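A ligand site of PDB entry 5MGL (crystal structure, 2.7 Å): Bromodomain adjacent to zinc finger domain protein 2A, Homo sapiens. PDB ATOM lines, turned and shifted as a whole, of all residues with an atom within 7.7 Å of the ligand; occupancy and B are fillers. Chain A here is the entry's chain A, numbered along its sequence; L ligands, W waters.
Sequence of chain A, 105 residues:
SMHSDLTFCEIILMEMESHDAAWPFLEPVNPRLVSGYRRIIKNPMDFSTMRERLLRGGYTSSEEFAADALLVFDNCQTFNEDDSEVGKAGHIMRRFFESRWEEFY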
ATOM      1  N   TRP A  23     -13.949 -25.866   0.955  1.00  0.00           N
ATOM      2  CA  TRP A  23     -12.617 -26.160   0.442  1.00  0.00           C
ATOM      3  C   TRP A  23     -12.516 -26.495  -1.061  1.00  0.00           C
ATOM      4  O   TRP A  23     -11.473 -26.264  -1.662  1.00  0.00           O
ATOM      5  CB  TRP A  23     -11.988 -27.300   1.255  1.00  0.00           C
ATOM      6  CG  TRP A  23     -12.780 -28.568   1.302  1.00  0.00           C
ATOM      7  CD1 TRP A  23     -13.761 -28.891   2.205  1.00  0.00           C
ATOM      8  CD2 TRP A  23     -12.665 -29.690   0.422  1.00  0.00           C
ATOM      9  NE1 TRP A  23     -14.258 -30.144   1.934  1.00  0.00           N
ATOM     10  CE2 TRP A  23     -13.608 -30.656   0.842  1.00  0.00           C
ATOM     11  CE3 TRP A  23     -11.865 -29.977  -0.694  1.00  0.00           C
ATOM     12  CZ2 TRP A  23     -13.768 -31.882   0.196  1.00  0.00           C
ATOM     13  CZ3 TRP A  23     -12.017 -31.192  -1.335  1.00  0.00           C
ATOM     14  CH2 TRP A  23     -12.964 -32.129  -0.892  1.00  0.00           C
ATOM     15  N   PRO A  24     -13.579 -27.050  -1.675  1.00  0.00           N
ATOM     16  CA  PRO A  24     -13.363 -27.284  -3.113  1.00  0.00           C
ATOM     17  C   PRO A  24     -13.550 -26.044  -3.980  1.00  0.00           C
ATOM     18  O   PRO A  24     -13.208 -26.073  -5.160  1.00  0.00           O
ATOM     19  CB  PRO A  24     -14.415 -28.338  -3.469  1.00  0.00           C
ATOM     20  CG  PRO A  24     -14.931 -28.856  -2.165  1.00  0.00           C
ATOM     21  CD  PRO A  24     -14.812 -27.712  -1.216  1.00  0.00           C
ATOM     22  N   PHE A  25     -14.075 -24.962  -3.412  1.00  0.00           N
ATOM     23  CA  PHE A  25     -14.495 -23.813  -4.214  1.00  0.00           C
ATOM     24  C   PHE A  25     -13.799 -22.510  -3.835  1.00  0.00           C
ATOM     25  O   PHE A  25     -14.185 -21.435  -4.304  1.00  0.00           O
ATOM     26  CB  PHE A  25     -16.009 -23.639  -4.122  1.00  0.00           C
ATOM     27  CG  PHE A  25     -16.759 -24.933  -4.064  1.00  0.00           C
ATOM     28  CD1 PHE A  25     -16.958 -25.684  -5.211  1.00  0.00           C
ATOM     29  CD2 PHE A  25     -17.249 -25.409  -2.859  1.00  0.00           C
ATOM     30  CE1 PHE A  25     -17.649 -26.882  -5.153  1.00  0.00           C
ATOM     31  CE2 PHE A  25     -17.941 -26.607  -2.801  1.00  0.00           C
ATOM     32  CZ  PHE A  25     -18.136 -27.338  -3.957  1.00  0.00           C
ATOM     33  N   LEU A  26     -12.773 -22.599  -2.994  1.00  0.00           N
ATOM     34  CA  LEU A  26     -12.022 -21.412  -2.589  1.00  0.00           C
ATOM     35  C   LEU A  26     -11.190 -20.864  -3.745  1.00  0.00           C
ATOM     36  O   LEU A  26     -11.142 -19.656  -3.965  1.00  0.00           O
ATOM     37  CB  LEU A  26     -11.120 -21.731  -1.393  1.00  0.00           C
ATOM     38  CG  LEU A  26     -11.820 -22.105  -0.091  1.00  0.00           C
ATOM     39  CD1 LEU A  26     -10.817 -22.415   1.001  1.00  0.00           C
ATOM     40  CD2 LEU A  26     -12.766 -20.993   0.343  1.00  0.00           C
ATOM     41  N   GLU A  27     -10.534 -21.764  -4.462  1.00  0.00           N
ATOM     42  CA  GLU A  27      -9.673 -21.384  -5.576  1.00  0.00           C
ATOM     43  C   GLU A  27     -10.128 -22.039  -6.878  1.00  0.00           C
ATOM     44  O   GLU A  27     -10.792 -23.074  -6.856  1.00  0.00           O
ATOM     45  CB  GLU A  27      -8.219 -21.760  -5.266  1.00  0.00           C
ATOM     46  CG  GLU A  27      -7.609 -20.991  -4.103  1.00  0.00           C
ATOM     47  CD  GLU A  27      -7.578 -19.493  -4.344  1.00  0.00           C
ATOM     48  OE1 GLU A  27      -7.407 -19.076  -5.518  1.00  0.00           O
ATOM     49  OE2 GLU A  27      -7.740 -18.727  -3.378  1.00  0.00           O
ATOM     50  N   PRO A  28      -9.773 -21.434  -8.026  1.00  0.00           N
ATOM     51  CA  PRO A  28     -10.135 -22.011  -9.321  1.00  0.00           C
ATOM     52  C   PRO A  28      -9.565 -23.417  -9.515  1.00  0.00           C
ATOM     53  O   PRO A  28      -8.435 -23.671  -9.091  1.00  0.00           O
ATOM     54  CB  PRO A  28      -9.535 -21.041 -10.334  1.00  0.00           C
ATOM     55  CG  PRO A  28      -9.373 -19.764  -9.594  1.00  0.00           C
ATOM     56  CD  PRO A  28      -9.060 -20.145  -8.182  1.00  0.00           C
ATOM     57  N   VAL A  29     -10.333 -24.296 -10.132  1.00  0.00           N
ATOM     58  CA  VAL A  29      -9.876 -25.653 -10.419  1.00  0.00           C
ATOM     59  C   VAL A  29      -8.675 -25.611 -11.364  1.00  0.00           C
ATOM     60  O   VAL A  29      -8.712 -24.940 -12.389  1.00  0.00           O
ATOM     61  CB  VAL A  29     -11.001 -26.505 -11.056  1.00  0.00           C
ATOM     62  CG1 VAL A  29     -10.451 -27.834 -11.542  1.00  0.00           C
ATOM     63  CG2 VAL A  29     -12.130 -26.710 -10.068  1.00  0.00           C
ATOM     64  N   ASN A  30      -7.610 -26.323 -10.992  1.00  0.00           N
ATOM     65  CA  ASN A  30      -6.428 -26.403 -11.838  1.00  0.00           C
ATOM     66  C   ASN A  30      -6.574 -27.510 -12.869  1.00  0.00           C
ATOM     67  O   ASN A  30      -6.506 -28.696 -12.529  1.00  0.00           O
ATOM     68  CB  ASN A  30      -5.179 -26.622 -10.985  1.00  0.00           C
ATOM     69  CG  ASN A  30      -3.890 -26.461 -11.776  1.00  0.00           C
ATOM     70  OD1 ASN A  30      -3.902 -26.151 -12.972  1.00  0.00           O
ATOM     71  ND2 ASN A  30      -2.759 -26.662 -11.110  1.00  0.00           N
ATOM     72  N   LEU A  33      -4.264 -30.443 -13.056  1.00  0.00           N
ATOM     73  CA  LEU A  33      -4.351 -31.436 -11.996  1.00  0.00           C
ATOM     74  C   LEU A  33      -5.634 -32.257 -12.092  1.00  0.00           C
ATOM     75  O   LEU A  33      -5.706 -33.364 -11.551  1.00  0.00           O
ATOM     76  CB  LEU A  33      -4.274 -30.754 -10.633  1.00  0.00           C
ATOM     77  CG  LEU A  33      -2.994 -29.961 -10.336  1.00  0.00           C
ATOM     78  CD1 LEU A  33      -3.099 -29.246  -9.001  1.00  0.00           C
ATOM     79  CD2 LEU A  33      -1.789 -30.885 -10.375  1.00  0.00           C
ATOM     80  N   VAL A  34      -6.635 -31.712 -12.765  1.00  0.00           N
ATOM     81  CA  VAL A  34      -7.933 -32.375 -12.862  1.00  0.00           C
ATOM     82  C   VAL A  34      -8.237 -32.767 -14.300  1.00  0.00           C
ATOM     83  O   VAL A  34      -8.599 -31.934 -15.131  1.00  0.00           O
ATOM     84  CB  VAL A  34      -9.052 -31.468 -12.324  1.00  0.00           C
ATOM     85  CG1 VAL A  34     -10.363 -32.221 -12.295  1.00  0.00           C
ATOM     86  CG2 VAL A  34      -8.707 -30.963 -10.938  1.00  0.00           C
ATOM     87  N   SER A  35      -8.105 -34.063 -14.588  1.00  0.00           N
ATOM     88  CA  SER A  35      -8.269 -34.582 -15.946  1.00  0.00           C
ATOM     89  C   SER A  35      -9.689 -34.415 -16.472  1.00  0.00           C
ATOM     90  O   SER A  35     -10.660 -34.850 -15.841  1.00  0.00           O
ATOM     91  CB  SER A  35      -7.875 -36.062 -15.988  1.00  0.00           C
ATOM     92  OG  SER A  35      -8.134 -36.609 -17.272  1.00  0.00           O
ATOM     93  N   TYR A  37     -11.412 -31.655 -16.943  1.00  0.00           N
ATOM     94  CA  TYR A  37     -12.178 -30.526 -16.422  1.00  0.00           C
ATOM     95  C   TYR A  37     -12.300 -29.401 -17.453  1.00  0.00           C
ATOM     96  O   TYR A  37     -13.322 -28.732 -17.518  1.00  0.00           O
ATOM     97  CB  TYR A  37     -11.545 -29.995 -15.131  1.00  0.00           C
ATOM     98  CG  TYR A  37     -12.476 -29.109 -14.346  1.00  0.00           C
ATOM     99  CD1 TYR A  37     -13.378 -29.656 -13.443  1.00  0.00           C
ATOM    100  CD2 TYR A  37     -12.473 -27.724 -14.515  1.00  0.00           C
ATOM    101  CE1 TYR A  37     -14.237 -28.855 -12.713  1.00  0.00           C
ATOM    102  CE2 TYR A  37     -13.342 -26.914 -13.790  1.00  0.00           C
ATOM    103  CZ  TYR A  37     -14.213 -27.488 -12.895  1.00  0.00           C
ATOM    104  OH  TYR A  37     -15.080 -26.698 -12.169  1.00  0.00           O
ATOM    105  N   ILE A  41     -16.307 -28.631 -18.239  1.00  0.00           N
ATOM    106  CA  ILE A  41     -16.798 -27.366 -17.702  1.00  0.00           C
ATOM    107  C   ILE A  41     -16.441 -26.176 -18.598  1.00  0.00           C
ATOM    108  O   ILE A  41     -15.267 -25.849 -18.761  1.00  0.00           O
ATOM    109  CB  ILE A  41     -16.253 -27.103 -16.287  1.00  0.00           C
ATOM    110  CG1 ILE A  41     -16.637 -28.254 -15.347  1.00  0.00           C
ATOM    111  CG2 ILE A  41     -16.786 -25.771 -15.747  1.00  0.00           C
ATOM    112  CD1 ILE A  41     -18.136 -28.461 -15.216  1.00  0.00           C
ATOM    113  N   MET A  45     -16.020 -21.363 -12.332  1.00  0.00           N
ATOM    114  CA  MET A  45     -16.250 -20.291 -11.379  1.00  0.00           C
ATOM    115  C   MET A  45     -15.992 -20.757  -9.955  1.00  0.00           C
ATOM    116  O   MET A  45     -16.350 -21.871  -9.579  1.00  0.00           O
ATOM    117  CB  MET A  45     -17.692 -19.761 -11.506  1.00  0.00           C
ATOM    118  CG  MET A  45     -18.015 -18.598 -10.587  1.00  0.00           C
ATOM    119  SD  MET A  45     -16.934 -17.175 -10.859  1.00  0.00           S
ATOM    120  CE  MET A  45     -17.271 -16.820 -12.580  1.00  0.00           C
ATOM    121  N   ASP A  46     -15.348 -19.907  -9.167  1.00  0.00           N
ATOM    122  CA  ASP A  46     -15.069 -20.201  -7.770  1.00  0.00           C
ATOM    123  C   ASP A  46     -15.285 -18.958  -6.916  1.00  0.00           C
ATOM    124  O   ASP A  46     -15.619 -17.898  -7.438  1.00  0.00           O
ATOM    125  CB  ASP A  46     -13.651 -20.732  -7.599  1.00  0.00           C
ATOM    126  CG  ASP A  46     -12.605 -19.685  -7.928  1.00  0.00           C
ATOM    127  OD1 ASP A  46     -12.452 -19.360  -9.115  1.00  0.00           O
ATOM    128  OD2 ASP A  46     -11.940 -19.204  -6.985  1.00  0.00           O
ATOM    129  N   VAL A  72     -21.077 -22.075  -9.700  1.00  0.00           N
ATOM    130  CA  VAL A  72     -20.118 -22.874  -8.946  1.00  0.00           C
ATOM    131  C   VAL A  72     -20.682 -24.259  -8.646  1.00  0.00           C
ATOM    132  O   VAL A  72     -20.004 -25.272  -8.812  1.00  0.00           O
ATOM    133  CB  VAL A  72     -19.738 -22.195  -7.615  1.00  0.00           C
ATOM    134  CG1 VAL A  72     -18.928 -23.127  -6.730  1.00  0.00           C
ATOM    135  CG2 VAL A  72     -18.983 -20.902  -7.873  1.00  0.00           C
ATOM    136  N   ASN A  75     -21.499 -26.360 -11.892  1.00  0.00           N
ATOM    137  CA  ASN A  75     -20.250 -26.943 -12.371  1.00  0.00           C
ATOM    138  C   ASN A  75     -19.837 -28.133 -11.528  1.00  0.00           C
ATOM    139  O   ASN A  75     -19.325 -29.135 -12.044  1.00  0.00           O
ATOM    140  CB  ASN A  75     -19.133 -25.897 -12.388  1.00  0.00           C
ATOM    141  CG  ASN A  75     -19.312 -24.868 -13.487  1.00  0.00           C
ATOM    142  OD1 ASN A  75     -20.088 -25.078 -14.422  1.00  0.00           O
ATOM    143  ND2 ASN A  75     -18.585 -23.766 -13.383  1.00  0.00           N
ATOM    144  N   CYS A  76     -20.056 -28.031 -10.211  1.00  0.00           N
ATOM    145  CA  CYS A  76     -19.710 -29.096  -9.286  1.00  0.00           C
ATOM    146  C   CYS A  76     -20.550 -30.340  -9.558  1.00  0.00           C
ATOM    147  O   CYS A  76     -20.034 -31.457  -9.532  1.00  0.00           O
ATOM    148  CB  CYS A  76     -19.930 -28.631  -7.841  1.00  0.00           C
ATOM    149  SG  CYS A  76     -19.421 -29.829  -6.584  1.00  0.00           S
ATOM    150  N   GLN A  77     -21.836 -30.139  -9.830  1.00  0.00           N
ATOM    151  CA  GLN A  77     -22.742 -31.249 -10.088  1.00  0.00           C
ATOM    152  C   GLN A  77     -22.507 -31.852 -11.473  1.00  0.00           C
ATOM    153  O   GLN A  77     -22.829 -33.008 -11.704  1.00  0.00           O
ATOM    154  CB  GLN A  77     -24.195 -30.788  -9.950  1.00  0.00           C
ATOM    155  CG  GLN A  77     -24.599 -30.461  -8.519  1.00  0.00           C
ATOM    156  CD  GLN A  77     -26.006 -29.887  -8.443  1.00  0.00           C
ATOM    157  OE1 GLN A  77     -26.975 -30.628  -8.311  1.00  0.00           O
ATOM    158  NE2 GLN A  77     -26.112 -28.572  -8.504  1.00  0.00           N
ATOM    159  N   PHE A  79     -19.414 -32.044 -13.071  1.00  0.00           N
ATOM    160  CA  PHE A  79     -18.150 -32.772 -13.128  1.00  0.00           C
ATOM    161  C   PHE A  79     -18.050 -33.858 -12.062  1.00  0.00           C
ATOM    162  O   PHE A  79     -17.456 -34.911 -12.320  1.00  0.00           O
ATOM    163  CB  PHE A  79     -16.981 -31.800 -12.996  1.00  0.00           C
ATOM    164  CG  PHE A  79     -15.648 -32.443 -13.239  1.00  0.00           C
ATOM    165  CD1 PHE A  79     -15.138 -32.548 -14.525  1.00  0.00           C
ATOM    166  CD2 PHE A  79     -14.899 -32.958 -12.189  1.00  0.00           C
ATOM    167  CE1 PHE A  79     -13.917 -33.141 -14.758  1.00  0.00           C
ATOM    168  CE2 PHE A  79     -13.678 -33.551 -12.422  1.00  0.00           C
ATOM    169  CZ  PHE A  79     -13.183 -33.647 -13.704  1.00  0.00           C
ATOM    170  N   ASN A  80     -18.596 -33.617 -10.881  1.00  0.00           N
ATOM    171  CA  ASN A  80     -18.444 -34.547  -9.770  1.00  0.00           C
ATOM    172  C   ASN A  80     -19.700 -35.363  -9.453  1.00  0.00           C
ATOM    173  O   ASN A  80     -20.825 -34.895  -9.628  1.00  0.00           O
ATOM    174  CB  ASN A  80     -17.974 -33.810  -8.512  1.00  0.00           C
ATOM    175  CG  ASN A  80     -16.643 -33.117  -8.714  1.00  0.00           C
ATOM    176  OD1 ASN A  80     -15.600 -33.755  -8.737  1.00  0.00           O
ATOM    177  ND2 ASN A  80     -16.684 -31.797  -8.853  1.00  0.00           N
ATOM    178  N   SER A  84     -19.336 -38.287  -4.382  1.00  0.00           N
ATOM    179  CA  SER A  84     -17.922 -37.946  -4.316  1.00  0.00           C
ATOM    180  C   SER A  84     -17.670 -36.949  -3.187  1.00  0.00           C
ATOM    181  O   SER A  84     -18.608 -36.338  -2.677  1.00  0.00           O
ATOM    182  CB  SER A  84     -17.432 -37.381  -5.642  1.00  0.00           C
ATOM    183  OG  SER A  84     -18.068 -36.146  -5.932  1.00  0.00           O
ATOM    184  N   VAL A  86     -15.985 -34.034  -3.302  1.00  0.00           N
ATOM    185  CA  VAL A  86     -16.287 -32.690  -3.784  1.00  0.00           C
ATOM    186  C   VAL A  86     -17.799 -32.519  -3.951  1.00  0.00           C
ATOM    187  O   VAL A  86     -18.354 -31.482  -3.593  1.00  0.00           O
ATOM    188  CB  VAL A  86     -15.578 -32.406  -5.129  1.00  0.00           C
ATOM    189  CG1 VAL A  86     -16.076 -31.101  -5.729  1.00  0.00           C
ATOM    190  CG2 VAL A  86     -14.076 -32.377  -4.937  1.00  0.00           C
ATOM    191  N   GLY A  87     -18.443 -33.557  -4.474  1.00  0.00           N
ATOM    192  CA  GLY A  87     -19.880 -33.540  -4.687  1.00  0.00           C
ATOM    193  C   GLY A  87     -20.663 -33.359  -3.396  1.00  0.00           C
ATOM    194  O   GLY A  87     -21.592 -32.550  -3.339  1.00  0.00           O
ATOM    195  N   GLY A  90     -20.173 -29.980  -2.202  1.00  0.00           N
ATOM    196  CA  GLY A  90     -20.896 -29.070  -3.075  1.00  0.00           C
ATOM    197  C   GLY A  90     -22.366 -28.971  -2.735  1.00  0.00           C
ATOM    198  O   GLY A  90     -22.949 -27.890  -2.799  1.00  0.00           O
HETATM  199  C1  LIG L   1     -14.936 -27.547  -7.484  1.00  0.00           C
HETATM  200  N1  LIG L   1     -13.914 -28.517  -7.430  1.00  0.00           N
HETATM  201  C2  LIG L   1     -13.887 -29.578  -8.412  1.00  0.00           C
HETATM  202  O1  LIG L   1     -14.751 -29.625  -9.274  1.00  0.00           O
HETATM  203  C3  LIG L   1     -12.779 -30.610  -8.337  1.00  0.00           C
HETATM  204  N2  LIG L   1     -11.630 -30.219  -7.808  1.00  0.00           N
HETATM  205  C4  LIG L   1     -10.597 -31.037  -7.697  1.00  0.00           C
HETATM  206  C5  LIG L   1     -10.703 -32.336  -8.135  1.00  0.00           C
HETATM  207  C6  LIG L   1     -11.916 -32.794  -8.701  1.00  0.00           C
HETATM  208  C7  LIG L   1     -12.993 -31.890  -8.810  1.00  0.00           C
HETATM  209 CL1  LIG L   1     -12.067 -34.440  -9.268  1.00  0.00          CL
HETATM  210  O   HOH W   1     -16.401 -27.838 -10.425  1.00  0.00           O
HETATM  211  O   HOH W   2     -17.511 -25.929  -9.025  1.00  0.00           O
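O of Cys 76 sits close to ND2 of Asn 80, 3.4 Å away.
The backbone carbonyl oxygen (O) of Val 86 sits at hydrogen-bond distance from the side-chain sulfur (SG) of Cys 76 (3.6 Å).
Water W1 bridges OH of Tyr 37 (2.5 Å) and O1 of the ligand (2.7 Å).
ND2 of Asn 80 lies within hydrogen-bond range of O1 of the ligand (2.9 Å).
The backbone carbonyl oxygen of Pro 24 sits close to a nitrogen (N1) of the ligand (3.4 Å).
Merely in contact with the ligand: Phe 25 (3.6 Å), Val 29 (3.7 Å), Val 34 (3.7 Å), Tyr 37 (3.6 Å), Phe 79 (3.7 Å) and Val 86 (3.8 Å).
Hydrophobic or aromatic side chains that line the ligand: Pro 24, Phe 25, Val 29, Val 34, Tyr 37, Phe 79 and Val 86.
Of the 25 residues printed, 8 come within 4 Å of the ligand.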
